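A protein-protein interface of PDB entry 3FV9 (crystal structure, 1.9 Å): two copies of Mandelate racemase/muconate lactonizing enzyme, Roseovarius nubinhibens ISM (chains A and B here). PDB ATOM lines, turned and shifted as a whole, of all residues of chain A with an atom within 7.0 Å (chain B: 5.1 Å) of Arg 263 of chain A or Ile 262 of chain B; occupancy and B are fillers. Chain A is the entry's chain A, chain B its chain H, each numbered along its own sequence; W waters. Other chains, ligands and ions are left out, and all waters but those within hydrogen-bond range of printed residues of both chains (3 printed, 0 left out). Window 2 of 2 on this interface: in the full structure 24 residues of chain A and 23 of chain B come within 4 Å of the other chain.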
ATOM      1  N   ASP A 257       4.890   5.661 -15.158  1.00  0.00           N
ATOM      2  CA  ASP A 257       5.291   4.466 -14.421  1.00  0.00           C
ATOM      3  C   ASP A 257       4.479   4.331 -13.131  1.00  0.00           C
ATOM      4  O   ASP A 257       4.018   3.248 -12.805  1.00  0.00           O
ATOM      5  CB  ASP A 257       6.809   4.453 -14.124  1.00  0.00           C
ATOM      6  CG  ASP A 257       7.661   4.235 -15.380  1.00  0.00           C
ATOM      7  OD1 ASP A 257       7.138   3.742 -16.404  1.00  0.00           O
ATOM      8  OD2 ASP A 257       8.861   4.580 -15.358  1.00  0.00           O
ATOM      9  N   LEU A 258       4.292   5.431 -12.410  1.00  0.00           N
ATOM     10  CA  LEU A 258       3.564   5.421 -11.137  1.00  0.00           C
ATOM     11  C   LEU A 258       2.077   5.110 -11.322  1.00  0.00           C
ATOM     12  O   LEU A 258       1.455   4.414 -10.509  1.00  0.00           O
ATOM     13  CB  LEU A 258       3.746   6.782 -10.459  1.00  0.00           C
ATOM     14  CG  LEU A 258       4.160   6.922  -9.002  1.00  0.00           C
ATOM     15  CD1 LEU A 258       5.033   5.775  -8.473  1.00  0.00           C
ATOM     16  CD2 LEU A 258       4.847   8.261  -8.864  1.00  0.00           C
ATOM     17  N   ILE A 259       1.510   5.630 -12.406  1.00  0.00           N
ATOM     18  CA  ILE A 259       0.121   5.350 -12.768  1.00  0.00           C
ATOM     19  C   ILE A 259      -0.067   3.854 -13.036  1.00  0.00           C
ATOM     20  O   ILE A 259      -1.034   3.246 -12.559  1.00  0.00           O
ATOM     21  CB  ILE A 259      -0.314   6.198 -14.006  1.00  0.00           C
ATOM     22  CG1 ILE A 259      -0.239   7.707 -13.694  1.00  0.00           C
ATOM     23  CG2 ILE A 259      -1.701   5.786 -14.521  1.00  0.00           C
ATOM     24  CD1 ILE A 259      -0.906   8.151 -12.368  1.00  0.00           C
ATOM     25  N   ALA A 260       0.867   3.269 -13.791  1.00  0.00           N
ATOM     26  CA  ALA A 260       0.879   1.822 -14.035  1.00  0.00           C
ATOM     27  C   ALA A 260       0.992   1.034 -12.739  1.00  0.00           C
ATOM     28  O   ALA A 260       0.318   0.012 -12.563  1.00  0.00           O
ATOM     29  CB  ALA A 260       2.020   1.437 -14.999  1.00  0.00           C
ATOM     30  N   ALA A 261       1.842   1.495 -11.829  1.00  0.00           N
ATOM     31  CA  ALA A 261       1.980   0.811 -10.548  1.00  0.00           C
ATOM     32  C   ALA A 261       0.687   0.846  -9.736  1.00  0.00           C
ATOM     33  O   ALA A 261       0.319  -0.153  -9.109  1.00  0.00           O
ATOM     34  CB  ALA A 261       3.164   1.387  -9.743  1.00  0.00           C
ATOM     35  N   ILE A 262       0.010   1.993  -9.735  1.00  0.00           N
ATOM     36  CA  ILE A 262      -1.292   2.134  -9.066  1.00  0.00           C
ATOM     37  C   ILE A 262      -2.324   1.219  -9.703  1.00  0.00           C
ATOM     38  O   ILE A 262      -3.039   0.487  -9.010  1.00  0.00           O
ATOM     39  CB  ILE A 262      -1.800   3.613  -9.099  1.00  0.00           C
ATOM     40  CG1 ILE A 262      -0.912   4.475  -8.202  1.00  0.00           C
ATOM     41  CG2 ILE A 262      -3.279   3.697  -8.654  1.00  0.00           C
ATOM     42  CD1 ILE A 262      -0.983   5.954  -8.498  1.00  0.00           C
ATOM     43  N   ARG A 263      -2.375   1.239 -11.034  1.00  0.00           N
ATOM     44  CA  ARG A 263      -3.309   0.403 -11.776  1.00  0.00           C
ATOM     45  C   ARG A 263      -3.139  -1.078 -11.438  1.00  0.00           C
ATOM     46  O   ARG A 263      -4.124  -1.814 -11.325  1.00  0.00           O
ATOM     47  CB  ARG A 263      -3.132   0.607 -13.286  1.00  0.00           C
ATOM     48  CG  ARG A 263      -4.119  -0.172 -14.140  1.00  0.00           C
ATOM     49  CD  ARG A 263      -5.513   0.498 -14.176  1.00  0.00           C
ATOM     50  NE  ARG A 263      -5.462   1.888 -14.638  1.00  0.00           N
ATOM     51  CZ  ARG A 263      -5.284   2.247 -15.911  1.00  0.00           C
ATOM     52  NH1 ARG A 263      -5.242   3.533 -16.236  1.00  0.00           N
ATOM     53  NH2 ARG A 263      -5.134   1.318 -16.862  1.00  0.00           N
ATOM     54  N   ASP A 264      -1.888  -1.494 -11.287  1.00  0.00           N
ATOM     55  CA  ASP A 264      -1.546  -2.887 -11.022  1.00  0.00           C
ATOM     56  C   ASP A 264      -1.458  -3.200  -9.541  1.00  0.00           C
ATOM     57  O   ASP A 264      -1.107  -4.332  -9.178  1.00  0.00           O
ATOM     58  CB  ASP A 264      -0.207  -3.249 -11.682  1.00  0.00           C
ATOM     59  CG  ASP A 264      -0.346  -3.591 -13.145  1.00  0.00           C
ATOM     60  OD1 ASP A 264       0.656  -3.473 -13.882  1.00  0.00           O
ATOM     61  OD2 ASP A 264      -1.447  -3.984 -13.560  1.00  0.00           O
ATOM     62  N   ASP A 265      -1.753  -2.210  -8.695  1.00  0.00           N
ATOM     63  CA  ASP A 265      -1.584  -2.323  -7.244  1.00  0.00           C
ATOM     64  C   ASP A 265      -0.230  -2.971  -6.902  1.00  0.00           C
ATOM     65  O   ASP A 265      -0.152  -3.940  -6.152  1.00  0.00           O
ATOM     66  CB  ASP A 265      -2.748  -3.105  -6.616  1.00  0.00           C
ATOM     67  CG  ASP A 265      -2.695  -3.118  -5.100  1.00  0.00           C
ATOM     68  OD1 ASP A 265      -2.074  -2.213  -4.503  1.00  0.00           O
ATOM     69  OD2 ASP A 265      -3.251  -4.055  -4.488  1.00  0.00           O
ATOM     70  N   LEU A 266       0.834  -2.414  -7.463  1.00  0.00           N
ATOM     71  CA  LEU A 266       2.115  -3.115  -7.518  1.00  0.00           C
ATOM     72  C   LEU A 266       3.051  -2.920  -6.321  1.00  0.00           C
ATOM     73  O   LEU A 266       3.933  -3.764  -6.075  1.00  0.00           O
ATOM     74  CB  LEU A 266       2.840  -2.729  -8.810  1.00  0.00           C
ATOM     75  CG  LEU A 266       4.057  -3.556  -9.226  1.00  0.00           C
ATOM     76  CD1 LEU A 266       3.765  -5.062  -9.249  1.00  0.00           C
ATOM     77  CD2 LEU A 266       4.542  -3.066 -10.572  1.00  0.00           C
ATOM     78  N   ILE A 289       1.698  12.278  -6.821  1.00  0.00           N
ATOM     79  CA  ILE A 289       1.020  11.025  -7.171  1.00  0.00           C
ATOM     80  C   ILE A 289       1.161  10.003  -6.036  1.00  0.00           C
ATOM     81  O   ILE A 289       0.179   9.425  -5.569  1.00  0.00           O
ATOM     82  CB  ILE A 289       1.560  10.455  -8.507  1.00  0.00           C
ATOM     83  CG1 ILE A 289       1.260  11.449  -9.647  1.00  0.00           C
ATOM     84  CG2 ILE A 289       0.962   9.052  -8.758  1.00  0.00           C
ATOM     85  CD1 ILE A 289       2.041  11.202 -10.970  1.00  0.00           C
ATOM     86  N   LEU B 258      -9.138  10.376  -7.179  1.00  0.00           N
ATOM     87  CA  LEU B 258      -8.527  10.205  -8.496  1.00  0.00           C
ATOM     88  C   LEU B 258      -7.713   8.910  -8.560  1.00  0.00           C
ATOM     89  O   LEU B 258      -7.715   8.211  -9.579  1.00  0.00           O
ATOM     90  CB  LEU B 258      -7.688  11.442  -8.841  1.00  0.00           C
ATOM     91  CG  LEU B 258      -7.591  11.952 -10.279  1.00  0.00           C
ATOM     92  CD1 LEU B 258      -8.901  11.844 -11.036  1.00  0.00           C
ATOM     93  CD2 LEU B 258      -7.095  13.391 -10.277  1.00  0.00           C
ATOM     94  N   ILE B 259      -7.038   8.571  -7.459  1.00  0.00           N
ATOM     95  CA  ILE B 259      -6.281   7.312  -7.364  1.00  0.00           C
ATOM     96  C   ILE B 259      -7.219   6.106  -7.475  1.00  0.00           C
ATOM     97  O   ILE B 259      -6.905   5.111  -8.147  1.00  0.00           O
ATOM     98  CB  ILE B 259      -5.456   7.241  -6.039  1.00  0.00           C
ATOM     99  CG1 ILE B 259      -4.434   8.390  -5.975  1.00  0.00           C
ATOM    100  CG2 ILE B 259      -4.787   5.881  -5.863  1.00  0.00           C
ATOM    101  CD1 ILE B 259      -3.555   8.527  -7.188  1.00  0.00           C
ATOM    102  N   ALA B 260      -8.365   6.198  -6.805  1.00  0.00           N
ATOM    103  CA  ALA B 260      -9.365   5.144  -6.889  1.00  0.00           C
ATOM    104  C   ALA B 260      -9.892   4.985  -8.320  1.00  0.00           C
ATOM    105  O   ALA B 260     -10.118   3.856  -8.749  1.00  0.00           O
ATOM    106  CB  ALA B 260     -10.505   5.379  -5.890  1.00  0.00           C
ATOM    107  N   ALA B 261     -10.062   6.096  -9.048  1.00  0.00           N
ATOM    108  CA  ALA B 261     -10.533   6.052 -10.444  1.00  0.00           C
ATOM    109  C   ALA B 261      -9.510   5.367 -11.334  1.00  0.00           C
ATOM    110  O   ALA B 261      -9.863   4.535 -12.171  1.00  0.00           O
ATOM    111  CB  ALA B 261     -10.877   7.442 -10.975  1.00  0.00           C
ATOM    112  N   ILE B 262      -8.234   5.673 -11.103  1.00  0.00           N
ATOM    113  CA  ILE B 262      -7.147   5.018 -11.814  1.00  0.00           C
ATOM    114  C   ILE B 262      -7.093   3.525 -11.511  1.00  0.00           C
ATOM    115  O   ILE B 262      -7.025   2.706 -12.431  1.00  0.00           O
ATOM    116  CB  ILE B 262      -5.784   5.685 -11.508  1.00  0.00           C
ATOM    117  CG1 ILE B 262      -5.812   7.124 -12.026  1.00  0.00           C
ATOM    118  CG2 ILE B 262      -4.624   4.854 -12.102  1.00  0.00           C
ATOM    119  CD1 ILE B 262      -4.651   7.967 -11.551  1.00  0.00           C
ATOM    120  N   ARG B 263      -7.135   3.174 -10.226  1.00  0.00           N
ATOM    121  CA  ARG B 263      -7.125   1.775  -9.799  1.00  0.00           C
ATOM    122  C   ARG B 263      -8.235   0.951 -10.449  1.00  0.00           C
ATOM    123  O   ARG B 263      -8.026  -0.204 -10.813  1.00  0.00           O
ATOM    124  CB  ARG B 263      -7.230   1.670  -8.263  1.00  0.00           C
ATOM    125  CG  ARG B 263      -7.452   0.250  -7.703  1.00  0.00           C
ATOM    126  CD  ARG B 263      -6.164  -0.593  -7.673  1.00  0.00           C
ATOM    127  NE  ARG B 263      -5.047   0.156  -7.087  1.00  0.00           N
ATOM    128  CZ  ARG B 263      -4.854   0.335  -5.781  1.00  0.00           C
ATOM    129  NH1 ARG B 263      -3.810   1.046  -5.369  1.00  0.00           N
ATOM    130  NH2 ARG B 263      -5.702  -0.177  -4.887  1.00  0.00           N
ATOM    131  N   ASP B 264      -9.416   1.550 -10.536  1.00  0.00           N
ATOM    132  CA  ASP B 264     -10.611   0.906 -11.094  1.00  0.00           C
ATOM    133  C   ASP B 264     -10.729   1.130 -12.605  1.00  0.00           C
ATOM    134  O   ASP B 264     -11.717   0.710 -13.221  1.00  0.00           O
ATOM    135  CB  ASP B 264     -11.861   1.494 -10.417  1.00  0.00           C
ATOM    136  CG  ASP B 264     -12.198   0.830  -9.096  1.00  0.00           C
ATOM    137  OD1 ASP B 264     -12.950   1.453  -8.306  1.00  0.00           O
ATOM    138  OD2 ASP B 264     -11.739  -0.305  -8.840  1.00  0.00           O
ATOM    139  N   ASP B 265      -9.736   1.800 -13.193  1.00  0.00           N
ATOM    140  CA  ASP B 265      -9.781   2.230 -14.605  1.00  0.00           C
ATOM    141  C   ASP B 265     -11.176   2.759 -14.964  1.00  0.00           C
ATOM    142  O   ASP B 265     -11.833   2.258 -15.877  1.00  0.00           O
ATOM    143  CB  ASP B 265      -9.376   1.078 -15.535  1.00  0.00           C
ATOM    144  CG  ASP B 265      -9.354   1.489 -17.010  1.00  0.00           C
ATOM    145  OD1 ASP B 265      -9.189   2.699 -17.314  1.00  0.00           O
ATOM    146  OD2 ASP B 265      -9.532   0.595 -17.865  1.00  0.00           O
ATOM    147  N   LEU B 266     -11.626   3.770 -14.222  1.00  0.00           N
ATOM    148  CA  LEU B 266     -13.045   4.108 -14.206  1.00  0.00           C
ATOM    149  C   LEU B 266     -13.432   5.171 -15.234  1.00  0.00           C
ATOM    150  O   LEU B 266     -14.587   5.231 -15.648  1.00  0.00           O
ATOM    151  CB  LEU B 266     -13.450   4.571 -12.795  1.00  0.00           C
ATOM    152  CG  LEU B 266     -14.936   4.747 -12.448  1.00  0.00           C
ATOM    153  CD1 LEU B 266     -15.710   3.472 -12.673  1.00  0.00           C
ATOM    154  CD2 LEU B 266     -15.086   5.177 -10.978  1.00  0.00           C
ATOM    155  N   ILE B 289      -1.760  14.279 -11.266  1.00  0.00           N
ATOM    156  CA  ILE B 289      -2.265  12.899 -11.317  1.00  0.00           C
ATOM    157  C   ILE B 289      -3.025  12.641 -12.631  1.00  0.00           C
ATOM    158  O   ILE B 289      -2.768  11.650 -13.317  1.00  0.00           O
ATOM    159  CB  ILE B 289      -3.168  12.539 -10.088  1.00  0.00           C
ATOM    160  CG1 ILE B 289      -2.388  12.629  -8.766  1.00  0.00           C
ATOM    161  CG2 ILE B 289      -3.740  11.113 -10.229  1.00  0.00           C
ATOM    162  CD1 ILE B 289      -3.298  12.962  -7.555  1.00  0.00           C
ATOM    163  N   ALA B 293      -1.876  10.121 -15.850  1.00  0.00           N
ATOM    164  CA  ALA B 293      -2.771   9.049 -16.332  1.00  0.00           C
ATOM    165  C   ALA B 293      -3.331   9.319 -17.745  1.00  0.00           C
ATOM    166  O   ALA B 293      -4.065   8.499 -18.305  1.00  0.00           O
ATOM    167  CB  ALA B 293      -3.915   8.807 -15.327  1.00  0.00           C
ATOM    168  N   MET B 295      -5.583  11.507 -18.539  1.00  0.00           N
ATOM    169  CA  MET B 295      -6.998  11.862 -18.446  1.00  0.00           C
ATOM    170  C   MET B 295      -7.156  13.295 -18.944  1.00  0.00           C
ATOM    171  O   MET B 295      -6.367  14.178 -18.581  1.00  0.00           O
ATOM    172  CB  MET B 295      -7.513  11.742 -16.998  1.00  0.00           C
ATOM    173  CG  MET B 295      -7.565  10.304 -16.392  1.00  0.00           C
ATOM    174  SD  MET B 295      -8.131  10.325 -14.653  1.00  0.00           S
ATOM    175  CE  MET B 295      -8.293   8.588 -14.317  1.00  0.00           C
HETATM  176  O   HOH W   1      -6.574  -0.683 -17.512  1.00  0.00           O
HETATM  177  O   HOH W   2      -6.316  -2.726  -4.987  1.00  0.00           O
HETATM  178  O   HOH W   3      -3.562   5.860 -17.811  1.00  0.00           O
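Water W1 bridges NH2 of Arg 263 of chain A (2.5 Å) and OD2 of Asp 265 of chain B (3.2 Å).
Water W2 lies within hydrogen-bond range of NH2 of Arg 263 of chain B and OD2 of Asp 265 of chain A.
Water W3 bridges the backbone carbonyl oxygen of Ala 293 of chain B and the guanidinium group of Arg 263 of chain A.
Printed residues of chain B that touch a printed residue of chain A: Ile 259, Ile 262, Arg 263, Ile 289 and Ala 293.
Hydrophobic or aromatic side chains of chain B that line the printed part of chain A: Ile 259, Ile 262, Ile 289 and Ala 293.
Along chain B the printed residues that touch a printed residue of chain A span positions 259 to 293.
Of the 11 printed residues of chain A, 5 touch a printed residue of chain B.
Hydrophobic or aromatic side chains of chain A that line the printed part of chain B: Ile 259, Ile 262 and Ile 289.
Among the printed residues, 8 pairs touch across the chains.
Among the printed residues, Asp or Glu carboxylates within 4 Å of a Lys or Arg side-chain nitrogen of the other chain: Asp 265 of chain A with Arg 263 of chain B.
Ile 259 of chain A touches Ile 262 of chain B.
Ile 259 of chain A touches Ala 293 of chain B.
Ile 262 of chain A touches Ile 259 of chain B.
CG2 of Ile 262 of chain B touches CG2 of Ile 262 of chain A (3.9 Å).
CG1 of Ile 289 of chain B touches CG1 of Ile 289 of chain A, 3.9 Å away.
Ile 259 of chain A touches Ile 262 of chain B, and with the chains exchanged Ile 262 of chain A touches Ile 259 of chain B.
Ile 262 of chain A touches its own counterpart, Ile 262 of chain B.
Ile 262 of chain A touches Arg 263 of chain B, and with the chains exchanged Arg 263 of chain A touches Ile 262 of chain B.
Ile 289 of chain B touches its own counterpart, Ile 289 of chain A.
10 positions are printed for both chains.
The guanidinium group (NE) of Arg 263 of chain B sits at hydrogen-bond distance from the backbone carbonyl oxygen (O) of Ile 262 of chain A (2.8 Å).
The guanidinium group (NE) of Arg 263 of chain A is in hydrogen-bond range of the backbone carbonyl oxygen (O) of Ile 262 of chain B (2.8 Å).
The side-chain carboxylate (OD1) of Asp 265 of chain A lies within salt-bridge range of the guanidinium group (NH1) of Arg 263 of chain B (3.8 Å).
Ile 262 of chain B touches just these residues of chain A: Ile 259, Ile 262 and Arg 263.
Printed residues of chain A within 4 Å of Ile 289 of chain B: Ile 289.
Of the printed residues of chain A, Ile 259 of chain B touches Ile 262.
Printed residues of chain B within 4 Å of Asp 265 of chain A: Arg 263 (3.8 Å).
Printed residues of chain A within 4 Å of Arg 263 of chain B: Ile 262 and Asp 265.
Printed residues of chain B within 4 Å of Ile 259 of chain A: Ile 262 and Ala 293.
Leu 258 of chain B touches none of the printed residues of chain A.
The nearest residue of chain B that does not touch Arg 263 of chain A is Asp 265 of chain B (4.1 Å).
The nearest printed residue of chain A that does not touch Ala 293 of chain B is Arg 263 of chain A (5.5 Å).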
